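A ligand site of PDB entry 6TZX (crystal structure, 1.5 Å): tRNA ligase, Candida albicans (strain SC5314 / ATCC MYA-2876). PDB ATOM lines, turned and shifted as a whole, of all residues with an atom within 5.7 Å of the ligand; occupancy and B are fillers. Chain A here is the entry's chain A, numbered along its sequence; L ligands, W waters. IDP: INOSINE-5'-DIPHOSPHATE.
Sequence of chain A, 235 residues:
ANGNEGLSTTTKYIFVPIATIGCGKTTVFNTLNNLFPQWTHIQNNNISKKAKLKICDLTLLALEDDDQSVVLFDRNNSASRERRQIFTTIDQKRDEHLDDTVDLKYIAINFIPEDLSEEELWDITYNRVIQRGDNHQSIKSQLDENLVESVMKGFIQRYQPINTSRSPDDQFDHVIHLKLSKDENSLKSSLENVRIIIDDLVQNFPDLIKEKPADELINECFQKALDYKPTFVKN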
ATOM      1  N   THR A  20      -1.655  34.497   8.015  1.00  0.00           N
ATOM      2  CA  THR A  20      -2.048  33.634   9.112  1.00  0.00           C
ATOM      3  C   THR A  20      -2.552  32.338   8.490  1.00  0.00           C
ATOM      4  O   THR A  20      -2.464  32.155   7.271  1.00  0.00           O
ATOM      5  CB  THR A  20      -3.071  34.344  10.015  1.00  0.00           C
ATOM      6  OG1 THR A  20      -4.204  34.743   9.236  1.00  0.00           O
ATOM      7  CG2 THR A  20      -2.462  35.583  10.663  1.00  0.00           C
ATOM      8  N   ILE A  21      -3.092  31.421   9.300  1.00  0.00           N
ATOM      9  CA  ILE A  21      -3.549  30.147   8.756  1.00  0.00           C
ATOM     10  C   ILE A  21      -4.787  30.353   7.883  1.00  0.00           C
ATOM     11  O   ILE A  21      -5.710  31.097   8.244  1.00  0.00           O
ATOM     12  CB  ILE A  21      -3.817  29.146   9.883  1.00  0.00           C
ATOM     13  CG1 ILE A  21      -2.523  28.799  10.618  1.00  0.00           C
ATOM     14  CG2 ILE A  21      -4.484  27.888   9.319  1.00  0.00           C
ATOM     15  CD1 ILE A  21      -2.725  27.889  11.798  1.00  0.00           C
ATOM     16  N   GLY A  22      -4.814  29.687   6.721  1.00  0.00           N
ATOM     17  CA  GLY A  22      -5.999  29.680   5.887  1.00  0.00           C
ATOM     18  C   GLY A  22      -6.199  30.901   5.026  1.00  0.00           C
ATOM     19  O   GLY A  22      -7.314  31.099   4.509  1.00  0.00           O
ATOM     20  N   CYS A  23      -5.163  31.713   4.857  1.00  0.00           N
ATOM     21  CA  CYS A  23      -5.247  32.884   3.977  1.00  0.00           C
ATOM     22  C   CYS A  23      -5.034  32.549   2.509  1.00  0.00           C
ATOM     23  O   CYS A  23      -5.164  33.453   1.671  1.00  0.00           O
ATOM     24  CB  CYS A  23      -4.201  33.920   4.392  1.00  0.00           C
ATOM     25  SG  CYS A  23      -4.528  34.698   5.959  1.00  0.00           S
ATOM     26  N   GLY A  24      -4.721  31.301   2.175  1.00  0.00           N
ATOM     27  CA  GLY A  24      -4.455  30.939   0.800  1.00  0.00           C
ATOM     28  C   GLY A  24      -2.988  30.759   0.458  1.00  0.00           C
ATOM     29  O   GLY A  24      -2.678  30.480  -0.717  1.00  0.00           O
ATOM     30  N   LYS A  25      -2.090  30.895   1.433  1.00  0.00           N
ATOM     31  CA  LYS A  25      -0.655  30.886   1.153  1.00  0.00           C
ATOM     32  C   LYS A  25      -0.209  29.599   0.453  1.00  0.00           C
ATOM     33  O   LYS A  25       0.409  29.650  -0.624  1.00  0.00           O
ATOM     34  CB  LYS A  25       0.107  31.100   2.462  1.00  0.00           C
ATOM     35  CG  LYS A  25       1.582  30.780   2.386  1.00  0.00           C
ATOM     36  CD  LYS A  25       2.221  30.864   3.786  1.00  0.00           C
ATOM     37  CE  LYS A  25       1.533  29.944   4.822  1.00  0.00           C
ATOM     38  NZ  LYS A  25       1.348  28.526   4.343  1.00  0.00           N
ATOM     39  N   THR A  26      -0.497  28.437   1.032  1.00  0.00           N
ATOM     40  CA  THR A  26      -0.053  27.181   0.422  1.00  0.00           C
ATOM     41  C   THR A  26      -0.724  26.966  -0.932  1.00  0.00           C
ATOM     42  O   THR A  26      -0.078  26.500  -1.882  1.00  0.00           O
ATOM     43  CB  THR A  26      -0.317  26.013   1.370  1.00  0.00           C
ATOM     44  OG1 THR A  26       0.475  26.195   2.551  1.00  0.00           O
ATOM     45  CG2 THR A  26       0.023  24.681   0.729  1.00  0.00           C
ATOM     46  N   THR A  27      -2.002  27.348  -1.051  1.00  0.00           N
ATOM     47  CA  THR A  27      -2.734  27.170  -2.313  1.00  0.00           C
ATOM     48  C   THR A  27      -2.134  28.027  -3.402  1.00  0.00           C
ATOM     49  O   THR A  27      -1.909  27.564  -4.521  1.00  0.00           O
ATOM     50  CB  THR A  27      -4.217  27.512  -2.115  1.00  0.00           C
ATOM     51  OG1 THR A  27      -4.755  26.701  -1.063  1.00  0.00           O
ATOM     52  CG2 THR A  27      -5.012  27.262  -3.388  1.00  0.00           C
ATOM     53  N   VAL A  28      -1.849  29.294  -3.089  1.00  0.00           N
ATOM     54  CA  VAL A  28      -1.254  30.202  -4.062  1.00  0.00           C
ATOM     55  C   VAL A  28       0.144  29.727  -4.470  1.00  0.00           C
ATOM     56  O   VAL A  28       0.477  29.696  -5.659  1.00  0.00           O
ATOM     57  CB  VAL A  28      -1.230  31.641  -3.519  1.00  0.00           C
ATOM     58  CG1 VAL A  28      -0.365  32.551  -4.403  1.00  0.00           C
ATOM     59  CG2 VAL A  28      -2.653  32.213  -3.434  1.00  0.00           C
ATOM     60  N   ASP A  74       7.582  29.022   1.981  1.00  0.00           N
ATOM     61  CA  ASP A  74       6.197  28.816   2.437  1.00  0.00           C
ATOM     62  C   ASP A  74       6.161  28.658   3.962  1.00  0.00           C
ATOM     63  O   ASP A  74       6.288  27.556   4.495  1.00  0.00           O
ATOM     64  CB  ASP A  74       5.569  27.629   1.724  1.00  0.00           C
ATOM     65  CG  ASP A  74       4.077  27.592   1.873  1.00  0.00           C
ATOM     66  OD1 ASP A  74       3.570  28.099   2.897  1.00  0.00           O
ATOM     67  OD2 ASP A  74       3.403  27.022   0.987  1.00  0.00           O
ATOM     68  N   ASN A  76       4.189  31.113   7.466  1.00  0.00           N
ATOM     69  CA  ASN A  76       3.230  32.205   7.707  1.00  0.00           C
ATOM     70  C   ASN A  76       3.921  33.554   7.882  1.00  0.00           C
ATOM     71  O   ASN A  76       3.484  34.560   7.308  1.00  0.00           O
ATOM     72  CB  ASN A  76       2.402  31.893   8.962  1.00  0.00           C
ATOM     73  CG  ASN A  76       1.474  30.758   8.740  1.00  0.00           C
ATOM     74  OD1 ASN A  76       0.409  30.910   8.144  1.00  0.00           O
ATOM     75  ND2 ASN A  76       1.900  29.583   9.192  1.00  0.00           N
ATOM     76  N   ARG A 128     -12.892  28.614   6.098  1.00  0.00           N
ATOM     77  CA  ARG A 128     -12.153  27.852   5.091  1.00  0.00           C
ATOM     78  C   ARG A 128     -11.532  26.609   5.700  1.00  0.00           C
ATOM     79  O   ARG A 128     -11.632  25.515   5.146  1.00  0.00           O
ATOM     80  CB  ARG A 128     -11.065  28.720   4.460  1.00  0.00           C
ATOM     81  CG  ARG A 128     -11.563  29.602   3.361  1.00  0.00           C
ATOM     82  CD  ARG A 128     -10.428  30.256   2.621  1.00  0.00           C
ATOM     83  NE  ARG A 128     -10.959  31.300   1.762  1.00  0.00           N
ATOM     84  CZ  ARG A 128     -10.222  32.163   1.092  1.00  0.00           C
ATOM     85  NH1 ARG A 128      -8.900  32.104   1.177  1.00  0.00           N
ATOM     86  NH2 ARG A 128     -10.806  33.092   0.343  1.00  0.00           N
ATOM     87  N   VAL A 129     -10.877  26.776   6.854  1.00  0.00           N
ATOM     88  CA  VAL A 129     -10.162  25.661   7.463  1.00  0.00           C
ATOM     89  C   VAL A 129     -11.128  24.566   7.877  1.00  0.00           C
ATOM     90  O   VAL A 129     -10.881  23.375   7.646  1.00  0.00           O
ATOM     91  CB  VAL A 129      -9.322  26.167   8.657  1.00  0.00           C
ATOM     92  CG1 VAL A 129      -8.798  25.005   9.489  1.00  0.00           C
ATOM     93  CG2 VAL A 129      -8.167  27.011   8.146  1.00  0.00           C
ATOM     94  N   ARG A 132     -13.041  23.230   4.374  1.00  0.00           N
ATOM     95  CA  ARG A 132     -12.242  22.677   3.282  1.00  0.00           C
ATOM     96  C   ARG A 132     -10.979  21.958   3.731  1.00  0.00           C
ATOM     97  O   ARG A 132     -10.389  21.224   2.928  1.00  0.00           O
ATOM     98  CB  ARG A 132     -11.853  23.796   2.297  1.00  0.00           C
ATOM     99  CG  ARG A 132     -13.053  24.437   1.574  1.00  0.00           C
ATOM    100  CD  ARG A 132     -12.594  25.429   0.513  1.00  0.00           C
ATOM    101  NE  ARG A 132     -13.683  25.836  -0.383  1.00  0.00           N
ATOM    102  CZ  ARG A 132     -13.838  25.384  -1.623  1.00  0.00           C
ATOM    103  NH1 ARG A 132     -12.982  24.518  -2.145  1.00  0.00           N
ATOM    104  NH2 ARG A 132     -14.859  25.810  -2.356  1.00  0.00           N
ATOM    105  N   GLY A 133     -10.544  22.146   4.976  1.00  0.00           N
ATOM    106  CA  GLY A 133      -9.346  21.487   5.472  1.00  0.00           C
ATOM    107  C   GLY A 133      -8.112  22.367   5.383  1.00  0.00           C
ATOM    108  O   GLY A 133      -8.046  23.331   4.619  1.00  0.00           O
ATOM    109  N   ASP A 134      -7.126  22.028   6.205  1.00  0.00           N
ATOM    110  CA  ASP A 134      -5.835  22.705   6.207  1.00  0.00           C
ATOM    111  C   ASP A 134      -4.800  21.707   6.695  1.00  0.00           C
ATOM    112  O   ASP A 134      -5.062  20.957   7.640  1.00  0.00           O
ATOM    113  CB  ASP A 134      -5.857  23.951   7.112  1.00  0.00           C
ATOM    114  CG  ASP A 134      -4.664  24.877   6.868  1.00  0.00           C
ATOM    115  OD1 ASP A 134      -3.523  24.518   7.211  1.00  0.00           O
ATOM    116  OD2 ASP A 134      -4.885  25.986   6.340  1.00  0.00           O
ATOM    117  N   ASN A 135      -3.645  21.678   6.037  1.00  0.00           N
ATOM    118  CA  ASN A 135      -2.647  20.675   6.337  1.00  0.00           C
ATOM    119  C   ASN A 135      -1.562  21.166   7.280  1.00  0.00           C
ATOM    120  O   ASN A 135      -0.567  20.466   7.497  1.00  0.00           O
ATOM    121  CB  ASN A 135      -2.033  20.156   5.030  1.00  0.00           C
ATOM    122  CG  ASN A 135      -3.082  19.576   4.098  1.00  0.00           C
ATOM    123  OD1 ASN A 135      -3.083  19.835   2.896  1.00  0.00           O
ATOM    124  ND2 ASN A 135      -4.024  18.814   4.668  1.00  0.00           N
ATOM    125  N   HIS A 136      -1.740  22.346   7.881  1.00  0.00           N
ATOM    126  CA  HIS A 136      -0.873  22.744   8.980  1.00  0.00           C
ATOM    127  C   HIS A 136      -0.855  21.635  10.022  1.00  0.00           C
ATOM    128  O   HIS A 136      -1.911  21.231  10.520  1.00  0.00           O
ATOM    129  CB  HIS A 136      -1.363  24.062   9.597  1.00  0.00           C
ATOM    130  CG  HIS A 136      -0.420  24.636  10.602  1.00  0.00           C
ATOM    131  ND1 HIS A 136       0.564  25.540  10.272  1.00  0.00           N
ATOM    132  CD2 HIS A 136      -0.310  24.430  11.936  1.00  0.00           C
ATOM    133  CE1 HIS A 136       1.250  25.860  11.354  1.00  0.00           C
ATOM    134  NE2 HIS A 136       0.737  25.207  12.376  1.00  0.00           N
ATOM    135  N   ASP A 183     -15.659  33.698  -0.541  1.00  0.00           N
ATOM    136  CA  ASP A 183     -16.095  33.160  -1.823  1.00  0.00           C
ATOM    137  C   ASP A 183     -17.494  33.656  -2.140  1.00  0.00           C
ATOM    138  O   ASP A 183     -18.418  33.537  -1.324  1.00  0.00           O
ATOM    139  CB  ASP A 183     -16.087  31.633  -1.807  1.00  0.00           C
ATOM    140  CG  ASP A 183     -14.702  31.021  -2.032  1.00  0.00           C
ATOM    141  OD1 ASP A 183     -13.696  31.740  -2.173  1.00  0.00           O
ATOM    142  OD2 ASP A 183     -14.669  29.777  -2.077  1.00  0.00           O
ATOM    143  N   LYS A 188     -12.935  33.274  -6.386  1.00  0.00           N
ATOM    144  CA  LYS A 188     -12.120  32.805  -5.283  1.00  0.00           C
ATOM    145  C   LYS A 188     -10.901  33.699  -5.190  1.00  0.00           C
ATOM    146  O   LYS A 188     -10.191  33.877  -6.183  1.00  0.00           O
ATOM    147  CB  LYS A 188     -11.702  31.343  -5.484  1.00  0.00           C
ATOM    148  CG  LYS A 188     -12.864  30.370  -5.332  1.00  0.00           C
ATOM    149  CD  LYS A 188     -12.429  28.933  -5.518  1.00  0.00           C
ATOM    150  CE  LYS A 188     -13.505  27.978  -5.006  1.00  0.00           C
ATOM    151  NZ  LYS A 188     -14.787  28.138  -5.745  1.00  0.00           N
ATOM    152  N   SER A 189     -10.676  34.301  -4.008  1.00  0.00           N
ATOM    153  CA  SER A 189      -9.598  35.286  -3.930  1.00  0.00           C
ATOM    154  C   SER A 189      -8.233  34.658  -4.181  1.00  0.00           C
ATOM    155  O   SER A 189      -7.316  35.347  -4.635  1.00  0.00           O
ATOM    156  CB  SER A 189      -9.616  36.052  -2.594  1.00  0.00           C
ATOM    157  OG  SER A 189      -9.652  35.197  -1.464  1.00  0.00           O
ATOM    158  N   SER A 190      -8.064  33.356  -3.922  1.00  0.00           N
ATOM    159  CA  SER A 190      -6.748  32.777  -4.147  1.00  0.00           C
ATOM    160  C   SER A 190      -6.416  32.753  -5.645  1.00  0.00           C
ATOM    161  O   SER A 190      -5.255  32.981  -6.027  1.00  0.00           O
ATOM    162  CB  SER A 190      -6.657  31.376  -3.546  1.00  0.00           C
ATOM    163  OG  SER A 190      -6.465  31.490  -2.149  1.00  0.00           O
ATOM    164  N   LEU A 191      -7.405  32.488  -6.520  1.00  0.00           N
ATOM    165  CA  LEU A 191      -7.144  32.551  -7.955  1.00  0.00           C
ATOM    166  C   LEU A 191      -6.920  34.002  -8.388  1.00  0.00           C
ATOM    167  O   LEU A 191      -6.011  34.282  -9.164  1.00  0.00           O
ATOM    168  CB  LEU A 191      -8.299  31.901  -8.745  1.00  0.00           C
ATOM    169  CG  LEU A 191      -8.197  31.948 -10.267  1.00  0.00           C
ATOM    170  CD1 LEU A 191      -6.837  31.422 -10.750  1.00  0.00           C
ATOM    171  CD2 LEU A 191      -9.335  31.176 -10.898  1.00  0.00           C
ATOM    172  N   PHE A 222      -4.397  26.275 -10.720  1.00  0.00           N
ATOM    173  CA  PHE A 222      -5.117  26.633  -9.501  1.00  0.00           C
ATOM    174  C   PHE A 222      -6.064  25.514  -9.075  1.00  0.00           C
ATOM    175  O   PHE A 222      -6.118  25.172  -7.885  1.00  0.00           O
ATOM    176  CB  PHE A 222      -5.873  27.938  -9.688  1.00  0.00           C
ATOM    177  CG  PHE A 222      -6.720  28.284  -8.515  1.00  0.00           C
ATOM    178  CD1 PHE A 222      -6.155  28.757  -7.351  1.00  0.00           C
ATOM    179  CD2 PHE A 222      -8.091  28.108  -8.567  1.00  0.00           C
ATOM    180  CE1 PHE A 222      -6.937  29.073  -6.249  1.00  0.00           C
ATOM    181  CE2 PHE A 222      -8.883  28.412  -7.482  1.00  0.00           C
ATOM    182  CZ  PHE A 222      -8.309  28.887  -6.337  1.00  0.00           C
ATOM    183  N   ALA A 225      -4.163  22.888  -7.345  1.00  0.00           N
ATOM    184  CA  ALA A 225      -3.737  23.292  -6.018  1.00  0.00           C
ATOM    185  C   ALA A 225      -4.908  23.308  -5.041  1.00  0.00           C
ATOM    186  O   ALA A 225      -4.769  22.891  -3.884  1.00  0.00           O
ATOM    187  CB  ALA A 225      -3.075  24.661  -6.079  1.00  0.00           C
ATOM    188  N   LEU A 226      -6.070  23.803  -5.493  1.00  0.00           N
ATOM    189  CA  LEU A 226      -7.250  23.836  -4.638  1.00  0.00           C
ATOM    190  C   LEU A 226      -7.671  22.434  -4.221  1.00  0.00           C
ATOM    191  O   LEU A 226      -8.095  22.222  -3.078  1.00  0.00           O
ATOM    192  CB  LEU A 226      -8.395  24.560  -5.377  1.00  0.00           C
ATOM    193  CG  LEU A 226      -9.607  24.964  -4.524  1.00  0.00           C
ATOM    194  CD1 LEU A 226      -9.234  26.068  -3.561  1.00  0.00           C
ATOM    195  CD2 LEU A 226     -10.739  25.414  -5.437  1.00  0.00           C
ATOM    196  N   ASP A 227      -7.550  21.455  -5.127  1.00  0.00           N
ATOM    197  CA  ASP A 227      -7.973  20.081  -4.863  1.00  0.00           C
ATOM    198  C   ASP A 227      -6.901  19.254  -4.175  1.00  0.00           C
ATOM    199  O   ASP A 227      -7.156  18.095  -3.854  1.00  0.00           O
ATOM    200  CB  ASP A 227      -8.371  19.357  -6.155  1.00  0.00           C
ATOM    201  CG  ASP A 227      -9.545  19.995  -6.861  1.00  0.00           C
ATOM    202  OD1 ASP A 227      -9.659  19.778  -8.084  1.00  0.00           O
ATOM    203  OD2 ASP A 227     -10.343  20.702  -6.204  1.00  0.00           O
HETATM  204  PB  IDP L   1      -2.333  27.326   4.441  1.00  0.00           P
HETATM  205  O1B IDP L   1      -1.428  26.118   4.578  1.00  0.00           O
HETATM  206  O2B IDP L   1      -2.937  27.692   5.781  1.00  0.00           O
HETATM  207  O3B IDP L   1      -1.613  28.477   3.810  1.00  0.00           O
HETATM  208  PA  IDP L   1      -4.401  27.624   2.514  1.00  0.00           P
HETATM  209  O1A IDP L   1      -3.749  27.786   1.154  1.00  0.00           O
HETATM  210  O2A IDP L   1      -4.767  28.904   3.212  1.00  0.00           O
HETATM  211  O3A IDP L   1      -3.487  26.733   3.493  1.00  0.00           O
HETATM  212  O5' IDP L   1      -5.704  26.694   2.333  1.00  0.00           O
HETATM  213  C5' IDP L   1      -6.594  26.501   3.423  1.00  0.00           C
HETATM  214  C4' IDP L   1      -7.886  25.935   2.843  1.00  0.00           C
HETATM  215  O4' IDP L   1      -8.539  26.963   2.108  1.00  0.00           O
HETATM  216  C3' IDP L   1      -7.641  24.795   1.865  1.00  0.00           C
HETATM  217  O3' IDP L   1      -8.646  23.790   2.083  1.00  0.00           O
HETATM  218  C2' IDP L   1      -7.800  25.442   0.507  1.00  0.00           C
HETATM  219  O2' IDP L   1      -8.221  24.545  -0.537  1.00  0.00           O
HETATM  220  C1' IDP L   1      -8.837  26.503   0.784  1.00  0.00           C
HETATM  221  N9  IDP L   1      -8.720  27.661  -0.110  1.00  0.00           N
HETATM  222  C8  IDP L   1      -7.581  28.216  -0.587  1.00  0.00           C
HETATM  223  N7  IDP L   1      -7.870  29.291  -1.343  1.00  0.00           N
HETATM  224  C5  IDP L   1      -9.220  29.458  -1.334  1.00  0.00           C
HETATM  225  C6  IDP L   1     -10.180  30.396  -1.919  1.00  0.00           C
HETATM  226  O6  IDP L   1      -9.803  31.361  -2.634  1.00  0.00           O
HETATM  227  N1  IDP L   1     -11.477  30.187  -1.640  1.00  0.00           N
HETATM  228  C2  IDP L   1     -11.889  29.164  -0.877  1.00  0.00           C
HETATM  229  N3  IDP L   1     -11.077  28.267  -0.289  1.00  0.00           N
HETATM  230  C4  IDP L   1      -9.744  28.385  -0.504  1.00  0.00           C
HETATM  231  O   HOH W   1      -2.700  23.568   3.999  1.00  0.00           O
HETATM  232  O   HOH W   2      -7.662  21.215   1.333  1.00  0.00           O
HETATM  233  O   HOH W   3      -5.728  23.926  -1.426  1.00  0.00           O
HETATM  234  O   HOH W   4      -2.441  30.984   4.675  1.00  0.00           O
HETATM  235  O   HOH W   5      -7.493  30.093   1.843  1.00  0.00           O
HETATM  236  O   HOH W   6     -10.509  23.174  -1.113  1.00  0.00           O
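The backbone NH (N) of Ser 190 lies within hydrogen-bond range of an oxygen (O6) of the ligand.
O of Leu 226 sits at hydrogen-bond distance from O2' of the ligand (3.4 Å).
O3' of the ligand is in hydrogen-bond range of O of Gly 133, 2.6 Å away.
OG1 of Thr 27 sits at hydrogen-bond distance from O1A of the ligand.
The backbone NH (N) of Lys 25 lies close to an oxygen (O3B) of the ligand (3.4 Å).
The side-chain amino group (NZ) of Lys 25 lies within salt-bridge range of an oxygen (O3B) of the ligand (3.0 Å).
An oxygen (O3') of the ligand lies close to the backbone carbonyl oxygen of Arg 132, at 3.2 Å.
A nitrogen (N1) of the ligand is in hydrogen-bond range of the side-chain carboxylate (OD1) of Asp 183 (2.8 Å).
O1A of the ligand lies within hydrogen-bond range of N of Thr 27 (2.8 Å).
The side-chain hydroxyl of Ser 190 lies within hydrogen-bond range of a nitrogen (N7) of the ligand (2.7 Å).
An oxygen (O2A) of the ligand is in hydrogen-bond range of the backbone NH of Cys 23 (3.3 Å).
OG1 of Thr 26 sits at hydrogen-bond distance from O1B of the ligand, 2.8 Å away.
N of Ser 189 sits at hydrogen-bond distance from O6 of the ligand (3.4 Å).
The backbone NH (N) of Gly 24 lies within hydrogen-bond range of an oxygen (O2A) of the ligand (2.6 Å).
An oxygen (O2B) of the ligand is in hydrogen-bond range of the backbone NH (N) of Gly 22, 2.9 Å away.
An oxygen (O2B) of the ligand lies close to the side-chain carboxylate (OD2) of Asp 134 (2.6 Å).
An oxygen (O3B) of the ligand is in hydrogen-bond range of the backbone NH (N) of Thr 26 (3.0 Å).
OG of Ser 189 lies within hydrogen-bond range of NH2 of Arg 128 (3.0 Å).
SG of Cys 23 is in hydrogen-bond range of OG1 of Thr 20.
The side-chain hydroxyl of Thr 26 is in hydrogen-bond range of the side-chain carboxylate of Asp 74.
OD2 of Asp 183 is in salt-bridge range of NH2 of Arg 132 (3.98 Å).
The side-chain amino group (NZ) of Lys 25 sits at hydrogen-bond distance from the side-chain hydroxyl (OG1) of Thr 26 (3.1 Å).
The side-chain carboxylate (OD1) of Asp 134 sits at hydrogen-bond distance from the backbone NH (N) of His 136 (2.9 Å).
The side-chain amino group of Lys 25 is in salt-bridge range of the side-chain carboxylate of Asp 74, 2.7 Å away.
Residues that only touch the ligand: Lys 188 (3.4 Å), Arg 128 (3.5 Å) and Ile 21 (3.9 Å).
16 residues have an atom within 4 Å of the ligand: Ile 21, Gly 22, Cys 23, Gly 24, Lys 25, Thr 26, Thr 27, Arg 128, Arg 132, Gly 133, Asp 134, Asp 183, Lys 188, Ser 189, Ser 190 and Leu 226.
Along chain A the residues within 4 Å of the ligand span positions 21 to 226.
The nearest printed residue that does not touch the ligand is Phe 222 (4.7 Å).
Water W3 lies within hydrogen-bond range of O2' of the ligand (2.7 Å), O of Ala 225 (2.8 Å), OG1 of Thr 27 (3.0 Å) and O of Leu 226 (3.4 Å).
Water W6 lies within hydrogen-bond range of O2' of the ligand (2.7 Å), NH1 of Arg 132 (3.0 Å) and O of Leu 226 (3.3 Å).
Water W2 lies within hydrogen-bond range of O3' of the ligand and O of Arg 132.
Water W1 lies within hydrogen-bond range of an oxygen (O1B) of the ligand (2.9 Å), the backbone NH of Asn 135 (2.9 Å) and the side-chain carboxylate of Asp 134 (3.4 Å).
Water W5 lies within hydrogen-bond range of NH1 of Arg 128 (2.5 Å), O of Gly 22 (2.9 Å), N of Gly 24 (3.0 Å) and O2A of the ligand (3.3 Å).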
